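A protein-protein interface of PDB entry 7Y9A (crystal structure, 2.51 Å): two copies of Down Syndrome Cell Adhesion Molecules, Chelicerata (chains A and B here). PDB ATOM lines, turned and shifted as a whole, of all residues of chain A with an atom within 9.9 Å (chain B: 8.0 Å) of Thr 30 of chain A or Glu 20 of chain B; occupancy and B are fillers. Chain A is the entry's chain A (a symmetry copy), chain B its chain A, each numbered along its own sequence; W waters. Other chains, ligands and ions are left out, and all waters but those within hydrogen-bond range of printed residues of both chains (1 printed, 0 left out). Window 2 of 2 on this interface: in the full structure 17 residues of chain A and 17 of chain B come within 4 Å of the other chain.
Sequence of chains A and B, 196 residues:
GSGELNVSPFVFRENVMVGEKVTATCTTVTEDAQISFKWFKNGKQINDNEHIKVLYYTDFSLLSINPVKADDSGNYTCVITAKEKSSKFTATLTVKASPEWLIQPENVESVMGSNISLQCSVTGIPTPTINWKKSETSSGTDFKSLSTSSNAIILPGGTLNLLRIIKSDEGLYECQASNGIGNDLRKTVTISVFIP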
ATOM      1  N   GLY A   3     -19.112  -8.384 -20.607  1.00  0.00           N
ATOM      2  CA  GLY A   3     -17.650  -8.412 -20.881  1.00  0.00           C
ATOM      3  C   GLY A   3     -16.910  -9.449 -20.064  1.00  0.00           C
ATOM      4  O   GLY A   3     -15.789  -9.211 -19.612  1.00  0.00           O
ATOM      5  N   GLU A   4     -17.538 -10.601 -19.871  1.00  0.00           N
ATOM      6  CA  GLU A   4     -16.958 -11.708 -19.126  1.00  0.00           C
ATOM      7  C   GLU A   4     -16.909 -12.943 -20.019  1.00  0.00           C
ATOM      8  O   GLU A   4     -17.346 -12.920 -21.171  1.00  0.00           O
ATOM      9  CB  GLU A   4     -17.755 -11.981 -17.849  1.00  0.00           C
ATOM     10  CG  GLU A   4     -19.219 -12.299 -18.079  1.00  0.00           C
ATOM     11  CD  GLU A   4     -19.948 -12.618 -16.786  1.00  0.00           C
ATOM     12  OE1 GLU A   4     -19.445 -12.224 -15.710  1.00  0.00           O
ATOM     13  OE2 GLU A   4     -21.022 -13.259 -16.841  1.00  0.00           O
ATOM     14  N   LEU A   5     -16.368 -14.034 -19.477  1.00  0.00           N
ATOM     15  CA  LEU A   5     -16.163 -15.266 -20.233  1.00  0.00           C
ATOM     16  C   LEU A   5     -16.740 -16.446 -19.457  1.00  0.00           C
ATOM     17  O   LEU A   5     -16.283 -16.748 -18.353  1.00  0.00           O
ATOM     18  CB  LEU A   5     -14.674 -15.488 -20.518  1.00  0.00           C
ATOM     19  CG  LEU A   5     -14.313 -16.837 -21.141  1.00  0.00           C
ATOM     20  CD1 LEU A   5     -15.139 -17.111 -22.385  1.00  0.00           C
ATOM     21  CD2 LEU A   5     -12.821 -16.873 -21.460  1.00  0.00           C
ATOM     22  N   ASN A   6     -17.749 -17.097 -20.030  1.00  0.00           N
ATOM     23  CA  ASN A   6     -18.415 -18.232 -19.407  1.00  0.00           C
ATOM     24  C   ASN A   6     -18.455 -19.383 -20.398  1.00  0.00           C
ATOM     25  O   ASN A   6     -18.830 -19.189 -21.560  1.00  0.00           O
ATOM     26  CB  ASN A   6     -19.836 -17.866 -18.972  1.00  0.00           C
ATOM     27  CG  ASN A   6     -19.856 -16.867 -17.837  1.00  0.00           C
ATOM     28  OD1 ASN A   6     -19.525 -17.201 -16.700  1.00  0.00           O
ATOM     29  ND2 ASN A   6     -20.243 -15.632 -18.138  1.00  0.00           N
ATOM     30  N   VAL A   7     -18.065 -20.569 -19.943  1.00  0.00           N
ATOM     31  CA  VAL A   7     -18.188 -21.779 -20.747  1.00  0.00           C
ATOM     32  C   VAL A   7     -19.641 -22.233 -20.719  1.00  0.00           C
ATOM     33  O   VAL A   7     -20.223 -22.419 -19.646  1.00  0.00           O
ATOM     34  CB  VAL A   7     -17.252 -22.877 -20.217  1.00  0.00           C
ATOM     35  CG1 VAL A   7     -17.329 -24.111 -21.106  1.00  0.00           C
ATOM     36  CG2 VAL A   7     -15.825 -22.358 -20.129  1.00  0.00           C
ATOM     37  N   SER A   8     -20.233 -22.403 -21.895  1.00  0.00           N
ATOM     38  CA  SER A   8     -21.617 -22.864 -21.969  1.00  0.00           C
ATOM     39  C   SER A   8     -21.727 -24.273 -21.401  1.00  0.00           C
ATOM     40  O   SER A   8     -20.938 -25.152 -21.780  1.00  0.00           O
ATOM     41  CB  SER A   8     -22.109 -22.836 -23.414  1.00  0.00           C
ATOM     42  OG  SER A   8     -23.463 -23.240 -23.494  1.00  0.00           O
ATOM     43  N   PRO A   9     -22.675 -24.543 -20.502  1.00  0.00           N
ATOM     44  CA  PRO A   9     -22.747 -25.874 -19.888  1.00  0.00           C
ATOM     45  C   PRO A   9     -22.996 -26.963 -20.922  1.00  0.00           C
ATOM     46  O   PRO A   9     -23.700 -26.765 -21.914  1.00  0.00           O
ATOM     47  CB  PRO A   9     -23.919 -25.762 -18.903  1.00  0.00           C
ATOM     48  CG  PRO A   9     -24.084 -24.269 -18.644  1.00  0.00           C
ATOM     49  CD  PRO A   9     -23.683 -23.612 -19.950  1.00  0.00           C
ATOM     50  N   THR A  27     -18.275 -24.456 -25.917  1.00  0.00           N
ATOM     51  CA  THR A  27     -18.382 -23.161 -26.568  1.00  0.00           C
ATOM     52  C   THR A  27     -18.628 -22.118 -25.486  1.00  0.00           C
ATOM     53  O   THR A  27     -18.827 -22.445 -24.313  1.00  0.00           O
ATOM     54  CB  THR A  27     -19.499 -23.145 -27.618  1.00  0.00           C
ATOM     55  OG1 THR A  27     -19.507 -21.875 -28.283  1.00  0.00           O
ATOM     56  CG2 THR A  27     -20.847 -23.388 -26.971  1.00  0.00           C
ATOM     57  N   THR A  28     -18.608 -20.854 -25.890  1.00  0.00           N
ATOM     58  CA  THR A  28     -18.862 -19.757 -24.970  1.00  0.00           C
ATOM     59  C   THR A  28     -20.348 -19.410 -24.955  1.00  0.00           C
ATOM     60  O   THR A  28     -21.098 -19.736 -25.878  1.00  0.00           O
ATOM     61  CB  THR A  28     -18.043 -18.524 -25.357  1.00  0.00           C
ATOM     62  OG1 THR A  28     -18.156 -18.292 -26.766  1.00  0.00           O
ATOM     63  CG2 THR A  28     -16.580 -18.723 -24.993  1.00  0.00           C
ATOM     64  N   VAL A  29     -20.768 -18.741 -23.881  1.00  0.00           N
ATOM     65  CA  VAL A  29     -22.156 -18.302 -23.778  1.00  0.00           C
ATOM     66  C   VAL A  29     -22.431 -17.183 -24.777  1.00  0.00           C
ATOM     67  O   VAL A  29     -23.408 -17.230 -25.533  1.00  0.00           O
ATOM     68  CB  VAL A  29     -22.469 -17.866 -22.336  1.00  0.00           C
ATOM     69  CG1 VAL A  29     -23.851 -17.247 -22.258  1.00  0.00           C
ATOM     70  CG2 VAL A  29     -22.343 -19.056 -21.388  1.00  0.00           C
ATOM     71  N   THR A  30     -21.579 -16.161 -24.787  1.00  0.00           N
ATOM     72  CA  THR A  30     -21.661 -15.065 -25.741  1.00  0.00           C
ATOM     73  C   THR A  30     -20.480 -15.146 -26.698  1.00  0.00           C
ATOM     74  O   THR A  30     -19.367 -15.499 -26.297  1.00  0.00           O
ATOM     75  CB  THR A  30     -21.668 -13.710 -25.029  1.00  0.00           C
ATOM     76  OG1 THR A  30     -22.715 -13.691 -24.051  1.00  0.00           O
ATOM     77  CG2 THR A  30     -21.891 -12.582 -26.027  1.00  0.00           C
ATOM     78  N   GLU A  31     -20.730 -14.828 -27.967  1.00  0.00           N
ATOM     79  CA  GLU A  31     -19.695 -14.937 -28.985  1.00  0.00           C
ATOM     80  C   GLU A  31     -18.502 -14.069 -28.619  1.00  0.00           C
ATOM     81  O   GLU A  31     -18.659 -12.891 -28.293  1.00  0.00           O
ATOM     82  CB  GLU A  31     -20.247 -14.508 -30.342  1.00  0.00           C
ATOM     83  CG  GLU A  31     -19.250 -14.611 -31.485  1.00  0.00           C
ATOM     84  CD  GLU A  31     -18.729 -16.024 -31.675  1.00  0.00           C
ATOM     85  OE1 GLU A  31     -17.668 -16.348 -31.100  1.00  0.00           O
ATOM     86  OE2 GLU A  31     -19.380 -16.810 -32.396  1.00  0.00           O
ATOM     87  N   ASP A  32     -17.311 -14.648 -28.665  1.00  0.00           N
ATOM     88  CA  ASP A  32     -16.101 -13.875 -28.441  1.00  0.00           C
ATOM     89  C   ASP A  32     -15.126 -13.929 -29.606  1.00  0.00           C
ATOM     90  O   ASP A  32     -14.351 -12.976 -29.786  1.00  0.00           O
ATOM     91  CB  ASP A  32     -15.402 -14.360 -27.137  1.00  0.00           C
ATOM     92  CG  ASP A  32     -14.261 -13.455 -26.711  1.00  0.00           C
ATOM     93  OD1 ASP A  32     -13.339 -13.312 -27.526  1.00  0.00           O
ATOM     94  OD2 ASP A  32     -14.273 -12.880 -25.596  1.00  0.00           O
ATOM     95  N   ALA A  33     -15.014 -15.078 -30.278  1.00  0.00           N
ATOM     96  CA  ALA A  33     -14.243 -15.203 -31.507  1.00  0.00           C
ATOM     97  C   ALA A  33     -12.750 -15.010 -31.297  1.00  0.00           C
ATOM     98  O   ALA A  33     -12.021 -14.774 -32.269  1.00  0.00           O
ATOM     99  CB  ALA A  33     -14.734 -14.189 -32.549  1.00  0.00           C
ATOM    100  N   GLN A  34     -12.274 -15.080 -30.058  1.00  0.00           N
ATOM    101  CA  GLN A  34     -10.855 -14.919 -29.757  1.00  0.00           C
ATOM    102  C   GLN A  34     -10.432 -15.933 -28.701  1.00  0.00           C
ATOM    103  O   GLN A  34      -9.786 -15.598 -27.709  1.00  0.00           O
ATOM    104  CB  GLN A  34     -10.565 -13.494 -29.294  1.00  0.00           C
ATOM    105  CG  GLN A  34     -10.531 -12.475 -30.434  1.00  0.00           C
ATOM    106  CD  GLN A  34      -9.159 -11.844 -30.606  1.00  0.00           C
ATOM    107  OE1 GLN A  34      -8.421 -11.668 -29.638  1.00  0.00           O
ATOM    108  NE2 GLN A  34      -8.813 -11.496 -31.842  1.00  0.00           N
ATOM    109  N   ILE A  35     -10.820 -17.194 -28.893  1.00  0.00           N
ATOM    110  CA  ILE A  35     -10.699 -18.210 -27.858  1.00  0.00           C
ATOM    111  C   ILE A  35      -9.916 -19.419 -28.363  1.00  0.00           C
ATOM    112  O   ILE A  35      -9.712 -19.618 -29.563  1.00  0.00           O
ATOM    113  CB  ILE A  35     -12.087 -18.654 -27.346  1.00  0.00           C
ATOM    114  CG1 ILE A  35     -12.899 -19.238 -28.511  1.00  0.00           C
ATOM    115  CG2 ILE A  35     -12.821 -17.489 -26.704  1.00  0.00           C
ATOM    116  CD1 ILE A  35     -14.370 -19.467 -28.202  1.00  0.00           C
ATOM    117  N   PHE A  37      -9.173 -23.784 -26.939  1.00  0.00           N
ATOM    118  CA  PHE A  37      -9.784 -24.837 -26.143  1.00  0.00           C
ATOM    119  C   PHE A  37      -8.759 -25.866 -25.685  1.00  0.00           C
ATOM    120  O   PHE A  37      -7.759 -26.123 -26.362  1.00  0.00           O
ATOM    121  CB  PHE A  37     -10.888 -25.568 -26.934  1.00  0.00           C
ATOM    122  CG  PHE A  37     -11.956 -24.661 -27.474  1.00  0.00           C
ATOM    123  CD1 PHE A  37     -13.040 -24.310 -26.691  1.00  0.00           C
ATOM    124  CD2 PHE A  37     -11.878 -24.163 -28.766  1.00  0.00           C
ATOM    125  CE1 PHE A  37     -14.023 -23.476 -27.180  1.00  0.00           C
ATOM    126  CE2 PHE A  37     -12.860 -23.327 -29.260  1.00  0.00           C
ATOM    127  CZ  PHE A  37     -13.934 -22.984 -28.466  1.00  0.00           C
ATOM    128  N   ASP A  59     -14.991 -21.360 -33.147  1.00  0.00           N
ATOM    129  CA  ASP A  59     -15.848 -20.960 -32.039  1.00  0.00           C
ATOM    130  C   ASP A  59     -16.326 -22.133 -31.191  1.00  0.00           C
ATOM    131  O   ASP A  59     -17.156 -21.936 -30.296  1.00  0.00           O
ATOM    132  CB  ASP A  59     -17.056 -20.179 -32.564  1.00  0.00           C
ATOM    133  CG  ASP A  59     -17.648 -20.790 -33.828  1.00  0.00           C
ATOM    134  OD1 ASP A  59     -17.065 -20.584 -34.915  1.00  0.00           O
ATOM    135  OD2 ASP A  59     -18.697 -21.468 -33.739  1.00  0.00           O
ATOM    136  N   ILE A  80     -11.569 -22.713 -21.621  1.00  0.00           N
ATOM    137  CA  ILE A  80     -11.524 -21.753 -22.718  1.00  0.00           C
ATOM    138  C   ILE A  80     -10.644 -20.588 -22.290  1.00  0.00           C
ATOM    139  O   ILE A  80     -10.792 -20.069 -21.179  1.00  0.00           O
ATOM    140  CB  ILE A  80     -12.933 -21.268 -23.100  1.00  0.00           C
ATOM    141  CG1 ILE A  80     -13.801 -22.454 -23.528  1.00  0.00           C
ATOM    142  CG2 ILE A  80     -12.861 -20.229 -24.204  1.00  0.00           C
ATOM    143  CD1 ILE A  80     -15.246 -22.087 -23.821  1.00  0.00           C
ATOM    144  N   ALA A  82      -9.360 -16.762 -23.476  1.00  0.00           N
ATOM    145  CA  ALA A  82      -9.569 -15.628 -24.383  1.00  0.00           C
ATOM    146  C   ALA A  82      -8.733 -14.434 -23.936  1.00  0.00           C
ATOM    147  O   ALA A  82      -9.226 -13.492 -23.312  1.00  0.00           O
ATOM    148  CB  ALA A  82     -11.068 -15.267 -24.461  1.00  0.00           C
ATOM    149  N   ARG B  13     -28.986 -25.173 -22.784  1.00  0.00           N
ATOM    150  CA  ARG B  13     -28.784 -24.732 -21.412  1.00  0.00           C
ATOM    151  C   ARG B  13     -30.028 -24.011 -20.900  1.00  0.00           C
ATOM    152  O   ARG B  13     -30.855 -23.515 -21.668  1.00  0.00           O
ATOM    153  CB  ARG B  13     -27.562 -23.823 -21.316  1.00  0.00           C
ATOM    154  CG  ARG B  13     -27.653 -22.554 -22.125  1.00  0.00           C
ATOM    155  CD  ARG B  13     -26.473 -21.634 -21.815  1.00  0.00           C
ATOM    156  NE  ARG B  13     -26.602 -20.344 -22.486  1.00  0.00           N
ATOM    157  CZ  ARG B  13     -26.167 -20.100 -23.718  1.00  0.00           C
ATOM    158  NH1 ARG B  13     -25.566 -21.058 -24.411  1.00  0.00           N
ATOM    159  NH2 ARG B  13     -26.333 -18.899 -24.254  1.00  0.00           N
ATOM    160  N   GLU B  14     -30.156 -23.964 -19.574  1.00  0.00           N
ATOM    161  CA  GLU B  14     -31.382 -23.461 -18.962  1.00  0.00           C
ATOM    162  C   GLU B  14     -31.614 -21.994 -19.303  1.00  0.00           C
ATOM    163  O   GLU B  14     -32.600 -21.640 -19.960  1.00  0.00           O
ATOM    164  CB  GLU B  14     -31.318 -23.655 -17.447  1.00  0.00           C
ATOM    165  CG  GLU B  14     -31.400 -25.102 -17.001  1.00  0.00           C
ATOM    166  CD  GLU B  14     -32.725 -25.744 -17.358  1.00  0.00           C
ATOM    167  OE1 GLU B  14     -32.846 -26.267 -18.486  1.00  0.00           O
ATOM    168  OE2 GLU B  14     -33.648 -25.726 -16.514  1.00  0.00           O
ATOM    169  N   ASN B  15     -30.711 -21.121 -18.861  1.00  0.00           N
ATOM    170  CA  ASN B  15     -30.941 -19.679 -18.913  1.00  0.00           C
ATOM    171  C   ASN B  15     -30.270 -19.099 -20.156  1.00  0.00           C
ATOM    172  O   ASN B  15     -29.170 -18.553 -20.107  1.00  0.00           O
ATOM    173  CB  ASN B  15     -30.423 -19.011 -17.643  1.00  0.00           C
ATOM    174  CG  ASN B  15     -31.228 -19.384 -16.416  1.00  0.00           C
ATOM    175  OD1 ASN B  15     -30.705 -19.978 -15.472  1.00  0.00           O
ATOM    176  ND2 ASN B  15     -32.511 -19.038 -16.421  1.00  0.00           N
ATOM    177  N   VAL B  16     -30.960 -19.226 -21.286  1.00  0.00           N
ATOM    178  CA  VAL B  16     -30.548 -18.586 -22.529  1.00  0.00           C
ATOM    179  C   VAL B  16     -31.225 -17.222 -22.613  1.00  0.00           C
ATOM    180  O   VAL B  16     -32.432 -17.109 -22.387  1.00  0.00           O
ATOM    181  CB  VAL B  16     -30.905 -19.453 -23.747  1.00  0.00           C
ATOM    182  CG1 VAL B  16     -30.424 -18.743 -25.013  1.00  0.00           C
ATOM    183  CG2 VAL B  16     -30.279 -20.815 -23.617  1.00  0.00           C
ATOM    184  N   MET B  17     -30.447 -16.182 -22.904  1.00  0.00           N
ATOM    185  CA  MET B  17     -30.959 -14.819 -22.977  1.00  0.00           C
ATOM    186  C   MET B  17     -30.584 -14.196 -24.314  1.00  0.00           C
ATOM    187  O   MET B  17     -29.604 -14.590 -24.952  1.00  0.00           O
ATOM    188  CB  MET B  17     -30.420 -13.965 -21.832  1.00  0.00           C
ATOM    189  CG  MET B  17     -31.148 -14.193 -20.521  1.00  0.00           C
ATOM    190  SD  MET B  17     -30.072 -14.060 -19.083  1.00  0.00           S
ATOM    191  CE  MET B  17     -29.463 -12.385 -19.275  1.00  0.00           C
ATOM    192  N   VAL B  18     -31.409 -13.240 -24.747  1.00  0.00           N
ATOM    193  CA  VAL B  18     -31.200 -12.591 -26.031  1.00  0.00           C
ATOM    194  C   VAL B  18     -29.799 -12.011 -26.096  1.00  0.00           C
ATOM    195  O   VAL B  18     -29.271 -11.481 -25.109  1.00  0.00           O
ATOM    196  CB  VAL B  18     -32.261 -11.499 -26.247  1.00  0.00           C
ATOM    197  CG1 VAL B  18     -33.621 -12.129 -26.535  1.00  0.00           C
ATOM    198  CG2 VAL B  18     -32.339 -10.586 -25.031  1.00  0.00           C
ATOM    199  N   GLY B  19     -29.186 -12.111 -27.273  1.00  0.00           N
ATOM    200  CA  GLY B  19     -27.836 -11.657 -27.483  1.00  0.00           C
ATOM    201  C   GLY B  19     -26.778 -12.719 -27.290  1.00  0.00           C
ATOM    202  O   GLY B  19     -25.656 -12.553 -27.782  1.00  0.00           O
ATOM    203  N   GLU B  20     -27.101 -13.804 -26.593  1.00  0.00           N
ATOM    204  CA  GLU B  20     -26.141 -14.867 -26.356  1.00  0.00           C
ATOM    205  C   GLU B  20     -26.074 -15.801 -27.564  1.00  0.00           C
ATOM    206  O   GLU B  20     -26.760 -15.614 -28.572  1.00  0.00           O
ATOM    207  CB  GLU B  20     -26.511 -15.638 -25.092  1.00  0.00           C
ATOM    208  CG  GLU B  20     -26.417 -14.821 -23.815  1.00  0.00           C
ATOM    209  CD  GLU B  20     -26.859 -15.595 -22.588  1.00  0.00           C
ATOM    210  OE1 GLU B  20     -27.502 -16.654 -22.754  1.00  0.00           O
ATOM    211  OE2 GLU B  20     -26.567 -15.145 -21.459  1.00  0.00           O
ATOM    212  N   LYS B  21     -25.235 -16.828 -27.452  1.00  0.00           N
ATOM    213  CA  LYS B  21     -25.028 -17.819 -28.499  1.00  0.00           C
ATOM    214  C   LYS B  21     -25.597 -19.156 -28.054  1.00  0.00           C
ATOM    215  O   LYS B  21     -25.538 -19.505 -26.868  1.00  0.00           O
ATOM    216  CB  LYS B  21     -23.537 -17.955 -28.818  1.00  0.00           C
ATOM    217  CG  LYS B  21     -23.180 -19.051 -29.799  1.00  0.00           C
ATOM    218  CD  LYS B  21     -21.659 -19.234 -29.861  1.00  0.00           C
ATOM    219  CE  LYS B  21     -21.209 -19.724 -31.225  1.00  0.00           C
ATOM    220  NZ  LYS B  21     -20.523 -21.053 -31.134  1.00  0.00           N
ATOM    221  N   VAL B  22     -26.151 -19.905 -29.008  1.00  0.00           N
ATOM    222  CA  VAL B  22     -26.746 -21.208 -28.731  1.00  0.00           C
ATOM    223  C   VAL B  22     -26.272 -22.218 -29.759  1.00  0.00           C
ATOM    224  O   VAL B  22     -26.325 -21.966 -30.980  1.00  0.00           O
ATOM    225  CB  VAL B  22     -28.287 -21.131 -28.681  1.00  0.00           C
ATOM    226  CG1 VAL B  22     -28.901 -22.462 -29.035  1.00  0.00           C
ATOM    227  CG2 VAL B  22     -28.743 -20.670 -27.285  1.00  0.00           C
ATOM    228  N   THR B  23     -25.862 -23.380 -29.291  1.00  0.00           N
ATOM    229  CA  THR B  23     -25.371 -24.453 -30.122  1.00  0.00           C
ATOM    230  C   THR B  23     -26.256 -25.658 -29.875  1.00  0.00           C
ATOM    231  O   THR B  23     -26.851 -25.784 -28.798  1.00  0.00           O
ATOM    232  CB  THR B  23     -23.903 -24.783 -29.771  1.00  0.00           C
ATOM    233  OG1 THR B  23     -23.769 -24.930 -28.347  1.00  0.00           O
ATOM    234  CG2 THR B  23     -22.941 -23.668 -30.209  1.00  0.00           C
ATOM    235  N   ILE B  65     -26.867 -20.753 -33.466  1.00  0.00           N
ATOM    236  CA  ILE B  65     -27.715 -19.567 -33.475  1.00  0.00           C
ATOM    237  C   ILE B  65     -26.968 -18.479 -32.717  1.00  0.00           C
ATOM    238  O   ILE B  65     -26.778 -18.581 -31.498  1.00  0.00           O
ATOM    239  CB  ILE B  65     -29.087 -19.831 -32.842  1.00  0.00           C
ATOM    240  CG1 ILE B  65     -29.702 -21.103 -33.424  1.00  0.00           C
ATOM    241  CG2 ILE B  65     -30.010 -18.644 -33.064  1.00  0.00           C
ATOM    242  CD1 ILE B  65     -30.999 -21.520 -32.744  1.00  0.00           C
ATOM    243  N   ASN B  66     -26.539 -17.440 -33.432  1.00  0.00           N
ATOM    244  CA  ASN B  66     -25.769 -16.373 -32.802  1.00  0.00           C
ATOM    245  C   ASN B  66     -25.835 -15.079 -33.605  1.00  0.00           C
ATOM    246  O   ASN B  66     -25.474 -15.069 -34.790  1.00  0.00           O
ATOM    247  CB  ASN B  66     -24.312 -16.814 -32.633  1.00  0.00           C
ATOM    248  CG  ASN B  66     -23.410 -15.694 -32.151  1.00  0.00           C
ATOM    249  OD1 ASN B  66     -23.735 -15.002 -31.191  1.00  0.00           O
ATOM    250  ND2 ASN B  66     -22.270 -15.512 -32.815  1.00  0.00           N
ATOM    251  N   PRO B  67     -26.292 -13.963 -33.001  1.00  0.00           N
ATOM    252  CA  PRO B  67     -26.854 -13.868 -31.641  1.00  0.00           C
ATOM    253  C   PRO B  67     -28.314 -14.300 -31.636  1.00  0.00           C
ATOM    254  O   PRO B  67     -28.989 -14.163 -32.659  1.00  0.00           O
ATOM    255  CB  PRO B  67     -26.707 -12.382 -31.278  1.00  0.00           C
ATOM    256  CG  PRO B  67     -26.116 -11.699 -32.518  1.00  0.00           C
ATOM    257  CD  PRO B  67     -26.275 -12.655 -33.672  1.00  0.00           C
ATOM    258  N   VAL B  68     -28.791 -14.817 -30.517  1.00  0.00           N
ATOM    259  CA  VAL B  68     -30.142 -15.356 -30.433  1.00  0.00           C
ATOM    260  C   VAL B  68     -31.119 -14.230 -30.116  1.00  0.00           C
ATOM    261  O   VAL B  68     -30.817 -13.323 -29.330  1.00  0.00           O
ATOM    262  CB  VAL B  68     -30.217 -16.476 -29.378  1.00  0.00           C
ATOM    263  CG1 VAL B  68     -30.135 -15.895 -27.983  1.00  0.00           C
ATOM    264  CG2 VAL B  68     -31.497 -17.289 -29.555  1.00  0.00           C
ATOM    265  N   LYS B  69     -32.294 -14.291 -30.731  1.00  0.00           N
ATOM    266  CA  LYS B  69     -33.381 -13.360 -30.468  1.00  0.00           C
ATOM    267  C   LYS B  69     -34.555 -14.105 -29.841  1.00  0.00           C
ATOM    268  O   LYS B  69     -34.574 -15.336 -29.765  1.00  0.00           O
ATOM    269  CB  LYS B  69     -33.828 -12.659 -31.755  1.00  0.00           C
ATOM    270  CG  LYS B  69     -32.715 -12.403 -32.756  1.00  0.00           C
ATOM    271  CD  LYS B  69     -33.186 -11.494 -33.893  1.00  0.00           C
ATOM    272  CE  LYS B  69     -34.436 -12.048 -34.573  1.00  0.00           C
ATOM    273  NZ  LYS B  69     -34.228 -13.433 -35.104  1.00  0.00           N
ATOM    274  N   ASP B  72     -36.283 -16.902 -31.834  1.00  0.00           N
ATOM    275  CA  ASP B  72     -35.679 -18.217 -32.002  1.00  0.00           C
ATOM    276  C   ASP B  72     -36.231 -19.265 -31.042  1.00  0.00           C
ATOM    277  O   ASP B  72     -35.779 -20.414 -31.082  1.00  0.00           O
ATOM    278  CB  ASP B  72     -34.161 -18.117 -31.835  1.00  0.00           C
ATOM    279  CG  ASP B  72     -33.510 -17.278 -32.922  1.00  0.00           C
ATOM    280  OD1 ASP B  72     -33.854 -17.473 -34.106  1.00  0.00           O
ATOM    281  OD2 ASP B  72     -32.656 -16.423 -32.594  1.00  0.00           O
ATOM    282  N   VAL B  95     -35.970 -18.616 -25.381  1.00  0.00           N
ATOM    283  CA  VAL B  95     -35.107 -17.451 -25.222  1.00  0.00           C
ATOM    284  C   VAL B  95     -35.760 -16.487 -24.241  1.00  0.00           C
ATOM    285  O   VAL B  95     -36.948 -16.164 -24.367  1.00  0.00           O
ATOM    286  CB  VAL B  95     -34.852 -16.776 -26.579  1.00  0.00           C
ATOM    287  CG1 VAL B  95     -33.731 -15.752 -26.459  1.00  0.00           C
ATOM    288  CG2 VAL B  95     -34.521 -17.821 -27.632  1.00  0.00           C
ATOM    289  N   LYS B  96     -34.989 -16.027 -23.262  1.00  0.00           N
ATOM    290  CA  LYS B  96     -35.473 -15.133 -22.221  1.00  0.00           C
ATOM    291  C   LYS B  96     -34.822 -13.761 -22.359  1.00  0.00           C
ATOM    292  O   LYS B  96     -33.834 -13.578 -23.075  1.00  0.00           O
ATOM    293  CB  LYS B  96     -35.198 -15.731 -20.836  1.00  0.00           C
ATOM    294  CG  LYS B  96     -35.619 -17.181 -20.711  1.00  0.00           C
ATOM    295  CD  LYS B  96     -35.848 -17.586 -19.264  1.00  0.00           C
ATOM    296  CE  LYS B  96     -36.498 -18.963 -19.181  1.00  0.00           C
ATOM    297  NZ  LYS B  96     -36.830 -19.346 -17.780  1.00  0.00           N
HETATM  298  O   HOH W   1     -23.182 -14.035 -28.881  1.00  0.00           O
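No position is printed for both chains.
NZ of Lys 21 of chain B lies within salt-bridge range of OD2 of Asp 59 of chain A (3.2 Å). NH1 of Arg 13 of chain B lies within hydrogen-bond range of OG of Ser 8 of chain A, at 3.2 Å. O of Val 29 of chain A lies within hydrogen-bond range of N of Lys 21 of chain B, 2.7 Å away. NZ of Lys 21 of chain B is in hydrogen-bond range of OG1 of Thr 27 of chain A, 3.1 Å away. The side-chain carboxylate (OE2) of Glu 31 of chain A lies within hydrogen-bond range of the side-chain amide nitrogen (ND2) of Asn 66 of chain B (3.2 Å).
Pro 9 of chain A touches Arg 13 of chain B. CG2 of Thr 27 of chain A touches OG1 of Thr 23 of chain B (3.6 Å). Arg 13 of chain B touches Val 29 of chain A. CD of Glu 20 of chain B touches CG1 of Val 29 of chain A, 3.4 Å away. Thr 30 of chain A touches Glu 20 of chain B (OG1 to CG, 3.9 Å). OE2 of Glu 31 of chain A touches CE of Lys 21 of chain B, 3.6 Å away.
Of chain B, only Glu 20 comes within 4 Å of Thr 30 of chain A. Glu 20 of chain B touches two residues of chain A. No residue of chain A comes within 4 Å of Val 16 of chain B. No residue of chain A comes within 4 Å of Gly 19 of chain B. No residue of chain A comes within 4 Å of Val 68 of chain B. Of the printed residues of chain A, Arg 13 of chain B touches Ser 8 (3.2 Å), Pro 9 (3.9 Å) and Val 29 (3.6 Å). Printed residues of chain A within 4 Å of Asn 66 of chain B: Glu 31. Of the printed residues of chain A, Thr 23 of chain B touches Thr 27. Printed residues of chain B within 4 Å of Glu 31 of chain A: Lys 21 (3.6 Å) and Asn 66 (3.2 Å). Printed residues of chain B within 4 Å of Ser 8 of chain A: Arg 13 (3.2 Å). The nearest residue of chain B that does not touch Thr 30 of chain A is Gly 19 of chain B (4.2 Å). The nearest residue of chain A that does not touch Glu 20 of chain B is Glu 31 of chain A (5.4 Å).
N of Met 17 of chain B sits at hydrogen-bond distance from OE1 of Glu 20 of chain B (3.0 Å). The side-chain hydroxyl (OG1) of Thr 28 of chain A is in hydrogen-bond range of the backbone carbonyl oxygen (O) of Thr 30 of chain A (3.1 Å). O of Glu 20 of chain B sits at hydrogen-bond distance from N of Val 68 of chain B, at 2.9 Å. The side-chain carboxylate (OE1) of Glu 31 of chain A lies within hydrogen-bond range of the backbone NH (N) of Ala 33 of chain A. The backbone carbonyl oxygen of Asn 6 of chain A sits at hydrogen-bond distance from the backbone NH of Val 29 of chain A (3.1 Å). NH2 of Arg 13 of chain B is in hydrogen-bond range of O of Lys 21 of chain B.
Water W1 lies within hydrogen-bond range of OD1 of Asn 66 of chain B, N of Glu 31 of chain A and O of Gly 19 of chain B.
Of the 20 printed residues of chain A, 7 touch a printed residue of chain B. Printed residues of chain A that touch a printed residue of chain B: Ser 8, Pro 9, Thr 27, Val 29, Thr 30, Glu 31 and Asp 59. Hydrophobic or aromatic side chains of chain A within 4 Å of the printed part of chain B: Pro 9 and Val 29. Among the printed residues, Asp or Glu carboxylates within 4 Å of a Lys or Arg side-chain nitrogen of the other chain: Asp 59 of chain A with Lys 21 of chain B (3.2 Å).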
